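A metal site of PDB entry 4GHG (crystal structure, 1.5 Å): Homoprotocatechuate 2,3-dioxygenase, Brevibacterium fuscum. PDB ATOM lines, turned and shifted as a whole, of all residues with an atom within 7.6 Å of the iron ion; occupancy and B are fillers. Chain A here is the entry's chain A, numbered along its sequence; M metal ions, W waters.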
ATOM      1  N   ASP A 154     -14.607  -2.357 -19.869  1.00  0.00           N
ATOM      2  CA  ASP A 154     -14.725  -2.163 -21.310  1.00  0.00           C
ATOM      3  C   ASP A 154     -13.605  -2.784 -22.158  1.00  0.00           C
ATOM      4  O   ASP A 154     -13.879  -3.401 -23.192  1.00  0.00           O
ATOM      5  CB  ASP A 154     -14.875  -0.694 -21.692  1.00  0.00           C
ATOM      6  CG  ASP A 154     -15.273  -0.532 -23.149  1.00  0.00           C
ATOM      7  OD1 ASP A 154     -16.462  -0.798 -23.485  1.00  0.00           O
ATOM      8  OD2 ASP A 154     -14.384  -0.161 -23.942  1.00  0.00           O
ATOM      9  N   HIS A 155     -12.359  -2.556 -21.757  1.00  0.00           N
ATOM     10  CA  HIS A 155     -11.231  -3.041 -22.569  1.00  0.00           C
ATOM     11  C   HIS A 155      -9.919  -3.068 -21.870  1.00  0.00           C
ATOM     12  O   HIS A 155      -9.745  -2.534 -20.794  1.00  0.00           O
ATOM     13  CB  HIS A 155     -11.088  -2.179 -23.862  1.00  0.00           C
ATOM     14  CG  HIS A 155     -10.727  -0.738 -23.620  1.00  0.00           C
ATOM     15  ND1 HIS A 155     -11.667   0.234 -23.531  1.00  0.00           N
ATOM     16  CD2 HIS A 155      -9.497  -0.099 -23.531  1.00  0.00           C
ATOM     17  CE1 HIS A 155     -11.054   1.425 -23.364  1.00  0.00           C
ATOM     18  NE2 HIS A 155      -9.731   1.234 -23.382  1.00  0.00           N
ATOM     19  N   PHE A 156      -8.967  -3.707 -22.537  1.00  0.00           N
ATOM     20  CA  PHE A 156      -7.572  -3.629 -22.194  1.00  0.00           C
ATOM     21  C   PHE A 156      -6.836  -2.872 -23.305  1.00  0.00           C
ATOM     22  O   PHE A 156      -7.338  -2.735 -24.436  1.00  0.00           O
ATOM     23  CB  PHE A 156      -6.948  -5.028 -22.113  1.00  0.00           C
ATOM     24  CG  PHE A 156      -7.733  -6.042 -21.301  1.00  0.00           C
ATOM     25  CD1 PHE A 156      -8.084  -5.805 -19.991  1.00  0.00           C
ATOM     26  CD2 PHE A 156      -8.104  -7.255 -21.866  1.00  0.00           C
ATOM     27  CE1 PHE A 156      -8.776  -6.758 -19.260  1.00  0.00           C
ATOM     28  CE2 PHE A 156      -8.799  -8.216 -21.140  1.00  0.00           C
ATOM     29  CZ  PHE A 156      -9.138  -7.948 -19.844  1.00  0.00           C
ATOM     30  N   ASN A 157      -5.633  -2.408 -23.004  1.00  0.00           N
ATOM     31  CA  ASN A 157      -4.754  -1.791 -24.001  1.00  0.00           C
ATOM     32  C   ASN A 157      -3.305  -2.250 -23.733  1.00  0.00           C
ATOM     33  O   ASN A 157      -2.795  -2.122 -22.622  1.00  0.00           O
ATOM     34  CB  ASN A 157      -4.915  -0.265 -24.003  1.00  0.00           C
ATOM     35  CG  ASN A 157      -4.162   0.393 -25.144  1.00  0.00           C
ATOM     36  OD1 ASN A 157      -2.962   0.228 -25.266  1.00  0.00           O
ATOM     37  ND2 ASN A 157      -4.861   1.153 -25.962  1.00  0.00           N
ATOM     38  N   TRP A 192      -7.176  -0.717 -32.758  1.00  0.00           N
ATOM     39  CA  TRP A 192      -8.235  -1.060 -31.829  1.00  0.00           C
ATOM     40  C   TRP A 192      -9.023  -2.189 -32.417  1.00  0.00           C
ATOM     41  O   TRP A 192      -9.379  -2.151 -33.589  1.00  0.00           O
ATOM     42  CB  TRP A 192      -9.153   0.145 -31.667  1.00  0.00           C
ATOM     43  CG  TRP A 192      -8.617   1.272 -30.805  1.00  0.00           C
ATOM     44  CD1 TRP A 192      -9.038   1.631 -29.527  1.00  0.00           C
ATOM     45  CD2 TRP A 192      -7.572   2.228 -31.133  1.00  0.00           C
ATOM     46  NE1 TRP A 192      -8.338   2.707 -29.056  1.00  0.00           N
ATOM     47  CE2 TRP A 192      -7.422   3.102 -29.971  1.00  0.00           C
ATOM     48  CE3 TRP A 192      -6.774   2.452 -32.255  1.00  0.00           C
ATOM     49  CZ2 TRP A 192      -6.515   4.142 -29.952  1.00  0.00           C
ATOM     50  CZ3 TRP A 192      -5.848   3.492 -32.208  1.00  0.00           C
ATOM     51  CH2 TRP A 192      -5.714   4.315 -31.092  1.00  0.00           C
ATOM     52  N   HIS A 200     -13.690  -1.631 -28.895  1.00  0.00           N
ATOM     53  CA  HIS A 200     -12.666  -2.636 -28.632  1.00  0.00           C
ATOM     54  C   HIS A 200     -12.859  -3.442 -27.393  1.00  0.00           C
ATOM     55  O   HIS A 200     -13.545  -3.016 -26.463  1.00  0.00           O
ATOM     56  CB  HIS A 200     -11.269  -2.029 -28.670  1.00  0.00           C
ATOM     57  CG  HIS A 200     -11.014  -0.867 -27.737  1.00  0.00           C
ATOM     58  ND1 HIS A 200     -11.913   0.126 -27.479  1.00  0.00           N
ATOM     59  CD2 HIS A 200      -9.843  -0.511 -27.065  1.00  0.00           C
ATOM     60  CE1 HIS A 200     -11.317   1.069 -26.674  1.00  0.00           C
ATOM     61  NE2 HIS A 200     -10.049   0.686 -26.462  1.00  0.00           N
ATOM     62  N   ALA A 203      -6.594  -3.450 -27.511  1.00  0.00           N
ATOM     63  CA  ALA A 203      -5.992  -2.508 -28.419  1.00  0.00           C
ATOM     64  C   ALA A 203      -4.495  -2.648 -28.308  1.00  0.00           C
ATOM     65  O   ALA A 203      -3.982  -3.138 -27.311  1.00  0.00           O
ATOM     66  CB  ALA A 203      -6.425  -1.080 -28.091  1.00  0.00           C
ATOM     67  N   THR A 205      -0.919  -0.494 -28.723  1.00  0.00           N
ATOM     68  CA  THR A 205      -0.220   0.779 -28.771  1.00  0.00           C
ATOM     69  C   THR A 205       1.241   0.460 -29.040  1.00  0.00           C
ATOM     70  O   THR A 205       1.837  -0.361 -28.337  1.00  0.00           O
ATOM     71  CB  THR A 205      -0.356   1.521 -27.422  1.00  0.00           C
ATOM     72  OG1 THR A 205      -1.750   1.736 -27.147  1.00  0.00           O
ATOM     73  CG2 THR A 205       0.430   2.832 -27.422  1.00  0.00           C
ATOM     74  N   HIS A 213      -0.774  -1.272 -21.099  1.00  0.00           N
ATOM     75  CA  HIS A 213      -0.962   0.160 -21.081  1.00  0.00           C
ATOM     76  C   HIS A 213      -1.993   0.567 -20.060  1.00  0.00           C
ATOM     77  O   HIS A 213      -1.716   1.410 -19.226  1.00  0.00           O
ATOM     78  CB  HIS A 213      -1.306   0.725 -22.452  1.00  0.00           C
ATOM     79  CG  HIS A 213      -1.064   2.198 -22.525  1.00  0.00           C
ATOM     80  ND1 HIS A 213      -1.934   3.080 -22.013  1.00  0.00           N
ATOM     81  CD2 HIS A 213       0.042   2.936 -22.952  1.00  0.00           C
ATOM     82  CE1 HIS A 213      -1.438   4.315 -22.142  1.00  0.00           C
ATOM     83  NE2 HIS A 213      -0.241   4.234 -22.730  1.00  0.00           N
ATOM     84  N   HIS A 214      -3.193  -0.019 -20.132  1.00  0.00           N
ATOM     85  CA  HIS A 214      -4.239   0.262 -19.141  1.00  0.00           C
ATOM     86  C   HIS A 214      -5.323  -0.770 -19.194  1.00  0.00           C
ATOM     87  O   HIS A 214      -5.396  -1.551 -20.147  1.00  0.00           O
ATOM     88  CB  HIS A 214      -4.847   1.686 -19.322  1.00  0.00           C
ATOM     89  CG  HIS A 214      -5.402   1.982 -20.710  1.00  0.00           C
ATOM     90  ND1 HIS A 214      -4.639   2.525 -21.689  1.00  0.00           N
ATOM     91  CD2 HIS A 214      -6.680   1.814 -21.253  1.00  0.00           C
ATOM     92  CE1 HIS A 214      -5.388   2.692 -22.814  1.00  0.00           C
ATOM     93  NE2 HIS A 214      -6.640   2.275 -22.538  1.00  0.00           N
ATOM     94  N   VAL A 215      -6.179  -0.714 -18.174  1.00  0.00           N
ATOM     95  CA  VAL A 215      -7.465  -1.396 -18.137  1.00  0.00           C
ATOM     96  C   VAL A 215      -8.511  -0.289 -18.082  1.00  0.00           C
ATOM     97  O   VAL A 215      -8.317   0.709 -17.373  1.00  0.00           O
ATOM     98  CB  VAL A 215      -7.558  -2.304 -16.894  1.00  0.00           C
ATOM     99  CG1 VAL A 215      -8.917  -2.976 -16.836  1.00  0.00           C
ATOM    100  CG2 VAL A 215      -6.419  -3.329 -16.897  1.00  0.00           C
ATOM    101  N   ALA A 216      -9.606  -0.458 -18.824  1.00  0.00           N
ATOM    102  CA  ALA A 216     -10.645   0.563 -18.902  1.00  0.00           C
ATOM    103  C   ALA A 216     -11.993   0.075 -18.384  1.00  0.00           C
ATOM    104  O   ALA A 216     -12.447  -1.016 -18.757  1.00  0.00           O
ATOM    105  CB  ALA A 216     -10.839   1.061 -20.341  1.00  0.00           C
ATOM    106  N   HIS A 248     -12.115  11.458 -26.855  1.00  0.00           N
ATOM    107  CA  HIS A 248     -11.219  10.825 -27.811  1.00  0.00           C
ATOM    108  C   HIS A 248     -11.623  11.113 -29.244  1.00  0.00           C
ATOM    109  O   HIS A 248     -12.816  11.261 -29.538  1.00  0.00           O
ATOM    110  CB  HIS A 248     -11.249   9.303 -27.646  1.00  0.00           C
ATOM    111  CG  HIS A 248     -10.446   8.785 -26.462  1.00  0.00           C
ATOM    112  ND1 HIS A 248      -9.135   9.093 -26.282  1.00  0.00           N
ATOM    113  CD2 HIS A 248     -10.780   7.853 -25.482  1.00  0.00           C
ATOM    114  CE1 HIS A 248      -8.665   8.421 -25.202  1.00  0.00           C
ATOM    115  NE2 HIS A 248      -9.662   7.668 -24.716  1.00  0.00           N
ATOM    116  N   SER A 251     -12.289   6.238 -31.352  1.00  0.00           N
ATOM    117  CA  SER A 251     -13.295   5.670 -30.435  1.00  0.00           C
ATOM    118  C   SER A 251     -14.453   6.612 -30.103  1.00  0.00           C
ATOM    119  O   SER A 251     -15.527   6.141 -29.747  1.00  0.00           O
ATOM    120  CB  SER A 251     -12.695   5.089 -29.132  1.00  0.00           C
ATOM    121  OG  SER A 251     -12.543   6.054 -28.118  1.00  0.00           O
ATOM    122  N   TYR A 255     -13.362  10.299 -21.779  1.00  0.00           N
ATOM    123  CA  TYR A 255     -12.300   9.538 -21.120  1.00  0.00           C
ATOM    124  C   TYR A 255     -11.553  10.302 -20.042  1.00  0.00           C
ATOM    125  O   TYR A 255     -11.599  11.528 -19.962  1.00  0.00           O
ATOM    126  CB  TYR A 255     -11.301   9.042 -22.180  1.00  0.00           C
ATOM    127  CG  TYR A 255     -10.355  10.136 -22.658  1.00  0.00           C
ATOM    128  CD1 TYR A 255     -10.625  10.870 -23.799  1.00  0.00           C
ATOM    129  CD2 TYR A 255      -9.180  10.420 -21.957  1.00  0.00           C
ATOM    130  CE1 TYR A 255      -9.753  11.862 -24.239  1.00  0.00           C
ATOM    131  CE2 TYR A 255      -8.295  11.392 -22.393  1.00  0.00           C
ATOM    132  CZ  TYR A 255      -8.595  12.132 -23.527  1.00  0.00           C
ATOM    133  OH  TYR A 255      -7.719  13.104 -23.978  1.00  0.00           O
ATOM    134  N   TYR A 257      -7.655   9.258 -17.637  1.00  0.00           N
ATOM    135  CA  TYR A 257      -6.637   8.292 -17.209  1.00  0.00           C
ATOM    136  C   TYR A 257      -6.102   8.688 -15.859  1.00  0.00           C
ATOM    137  O   TYR A 257      -5.663   9.825 -15.655  1.00  0.00           O
ATOM    138  CB  TYR A 257      -5.457   8.248 -18.188  1.00  0.00           C
ATOM    139  CG  TYR A 257      -5.847   7.828 -19.594  1.00  0.00           C
ATOM    140  CD1 TYR A 257      -5.917   6.506 -19.969  1.00  0.00           C
ATOM    141  CD2 TYR A 257      -6.139   8.783 -20.549  1.00  0.00           C
ATOM    142  CE1 TYR A 257      -6.266   6.127 -21.254  1.00  0.00           C
ATOM    143  CE2 TYR A 257      -6.487   8.434 -21.841  1.00  0.00           C
ATOM    144  CZ  TYR A 257      -6.574   7.103 -22.178  1.00  0.00           C
ATOM    145  OH  TYR A 257      -6.917   6.770 -23.459  1.00  0.00           O
ATOM    146  N   GLU A 267      -8.208   3.621 -17.228  1.00  0.00           N
ATOM    147  CA  GLU A 267      -9.003   4.555 -17.995  1.00  0.00           C
ATOM    148  C   GLU A 267     -10.473   4.432 -17.559  1.00  0.00           C
ATOM    149  O   GLU A 267     -10.971   3.320 -17.333  1.00  0.00           O
ATOM    150  CB  GLU A 267      -8.897   4.266 -19.490  1.00  0.00           C
ATOM    151  CG  GLU A 267      -9.573   5.326 -20.351  1.00  0.00           C
ATOM    152  CD  GLU A 267      -9.503   5.001 -21.831  1.00  0.00           C
ATOM    153  OE1 GLU A 267      -8.974   3.934 -22.144  1.00  0.00           O
ATOM    154  OE2 GLU A 267      -9.968   5.777 -22.680  1.00  0.00           O
ATOM    155  N   ILE A 268     -11.159   5.584 -17.493  1.00  0.00           N
ATOM    156  CA  ILE A 268     -12.585   5.668 -17.341  1.00  0.00           C
ATOM    157  C   ILE A 268     -13.087   6.163 -18.679  1.00  0.00           C
ATOM    158  O   ILE A 268     -12.471   7.054 -19.265  1.00  0.00           O
ATOM    159  CB  ILE A 268     -13.040   6.560 -16.175  1.00  0.00           C
ATOM    160  CG1 ILE A 268     -12.096   6.466 -14.962  1.00  0.00           C
ATOM    161  CG2 ILE A 268     -14.496   6.213 -15.808  1.00  0.00           C
ATOM    162  CD1 ILE A 268     -12.026   5.108 -14.335  1.00  0.00           C
ATOM    163  N   TYR A 269     -14.171   5.563 -19.170  1.00  0.00           N
ATOM    164  CA  TYR A 269     -14.557   5.621 -20.591  1.00  0.00           C
ATOM    165  C   TYR A 269     -16.075   5.592 -20.724  1.00  0.00           C
ATOM    166  O   TYR A 269     -16.758   4.916 -19.957  1.00  0.00           O
ATOM    167  CB  TYR A 269     -13.938   4.374 -21.236  1.00  0.00           C
ATOM    168  CG  TYR A 269     -14.065   4.096 -22.722  1.00  0.00           C
ATOM    169  CD1 TYR A 269     -13.040   4.469 -23.605  1.00  0.00           C
ATOM    170  CD2 TYR A 269     -15.121   3.342 -23.224  1.00  0.00           C
ATOM    171  CE1 TYR A 269     -13.099   4.109 -24.952  1.00  0.00           C
ATOM    172  CE2 TYR A 269     -15.205   3.029 -24.573  1.00  0.00           C
ATOM    173  CZ  TYR A 269     -14.175   3.392 -25.426  1.00  0.00           C
ATOM    174  OH  TYR A 269     -14.243   3.039 -26.759  1.00  0.00           O
ATOM    175  N   ARG A 293      -6.312  11.734 -30.704  1.00  0.00           N
ATOM    176  CA  ARG A 293      -6.287  11.173 -29.363  1.00  0.00           C
ATOM    177  C   ARG A 293      -7.162  11.944 -28.415  1.00  0.00           C
ATOM    178  O   ARG A 293      -7.981  11.352 -27.721  1.00  0.00           O
ATOM    179  CB  ARG A 293      -4.862  11.023 -28.835  1.00  0.00           C
ATOM    180  CG  ARG A 293      -4.154   9.860 -29.537  1.00  0.00           C
ATOM    181  CD  ARG A 293      -2.970   9.350 -28.753  1.00  0.00           C
ATOM    182  NE  ARG A 293      -2.360   8.166 -29.376  1.00  0.00           N
ATOM    183  CZ  ARG A 293      -2.760   6.904 -29.236  1.00  0.00           C
ATOM    184  NH1 ARG A 293      -3.808   6.586 -28.494  1.00  0.00           N
ATOM    185  NH2 ARG A 293      -2.071   5.928 -29.832  1.00  0.00           N
ATOM    186  N   TRP A 304       2.231   9.320 -20.896  1.00  0.00           N
ATOM    187  CA  TRP A 304       1.175   8.477 -21.452  1.00  0.00           C
ATOM    188  C   TRP A 304       1.753   7.562 -22.500  1.00  0.00           C
ATOM    189  O   TRP A 304       1.324   6.403 -22.641  1.00  0.00           O
ATOM    190  CB  TRP A 304       0.028   9.340 -22.015  1.00  0.00           C
ATOM    191  CG  TRP A 304      -1.218   8.527 -22.248  1.00  0.00           C
ATOM    192  CD1 TRP A 304      -2.245   8.259 -21.350  1.00  0.00           C
ATOM    193  CD2 TRP A 304      -1.573   7.810 -23.461  1.00  0.00           C
ATOM    194  NE1 TRP A 304      -3.186   7.460 -21.918  1.00  0.00           N
ATOM    195  CE2 TRP A 304      -2.839   7.136 -23.173  1.00  0.00           C
ATOM    196  CE3 TRP A 304      -0.987   7.634 -24.702  1.00  0.00           C
ATOM    197  CZ2 TRP A 304      -3.484   6.351 -24.127  1.00  0.00           C
ATOM    198  CZ3 TRP A 304      -1.634   6.844 -25.647  1.00  0.00           C
ATOM    199  CH2 TRP A 304      -2.845   6.202 -25.361  1.00  0.00           C
HETATM  200 FE    FE M   1      -8.322   2.841 -23.792  1.00  0.00          FE
HETATM  201  O   HOH W   1      -9.821   3.916 -24.811  1.00  0.00           O
HETATM  202  O   HOH W   2      -7.731   1.765 -25.543  1.00  0.00           O
HETATM  203  O   HOH W   3      -7.108   4.499 -24.541  1.00  0.00           O
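OE2 of Glu 267 is in hydrogen-bond range of OH of Tyr 257, 3.3 Å away.
OE2 of Glu 267 sits at hydrogen-bond distance from NE2 of His 248.
The backbone NH (N) of Glu 267 is in hydrogen-bond range of the backbone carbonyl oxygen (O) of Val 215 (2.9 Å).
N of Asn 157 is in hydrogen-bond range of O of His 214.
ND1 of His 213 lies within hydrogen-bond range of ND1 of His 214, 2.8 Å away.
NE2 of His 200 sits close to ND1 of His 155 (3.4 Å).
The backbone NH of Ala 216 sits at hydrogen-bond distance from the backbone carbonyl oxygen of His 155 (2.9 Å).
A ring nitrogen (ND1) of His 155 sits at hydrogen-bond distance from the side-chain carboxylate (OD2) of Asp 154 (2.8 Å).
Residues that only touch the iron ion: His 200.
Of the 21 residues printed, 4 come within 4 Å of the iron ion.
OE1 of Glu 267 is bound to the iron ion (2.1 Å).
Water W1 binds the iron ion, at 2.1 Å.
Water W2 binds the iron ion, 2.1 Å away.
The iron ion is bound by NE2 of His 214, at 2.2 Å.
The iron ion is bound by NE2 of His 155 (2.2 Å).
The iron ion is bound by water W3 (2.2 Å).
Water W2 lies within hydrogen-bond range of NE2 of His 200 (2.7 Å) and ND2 of Asn 157 (3.0 Å).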
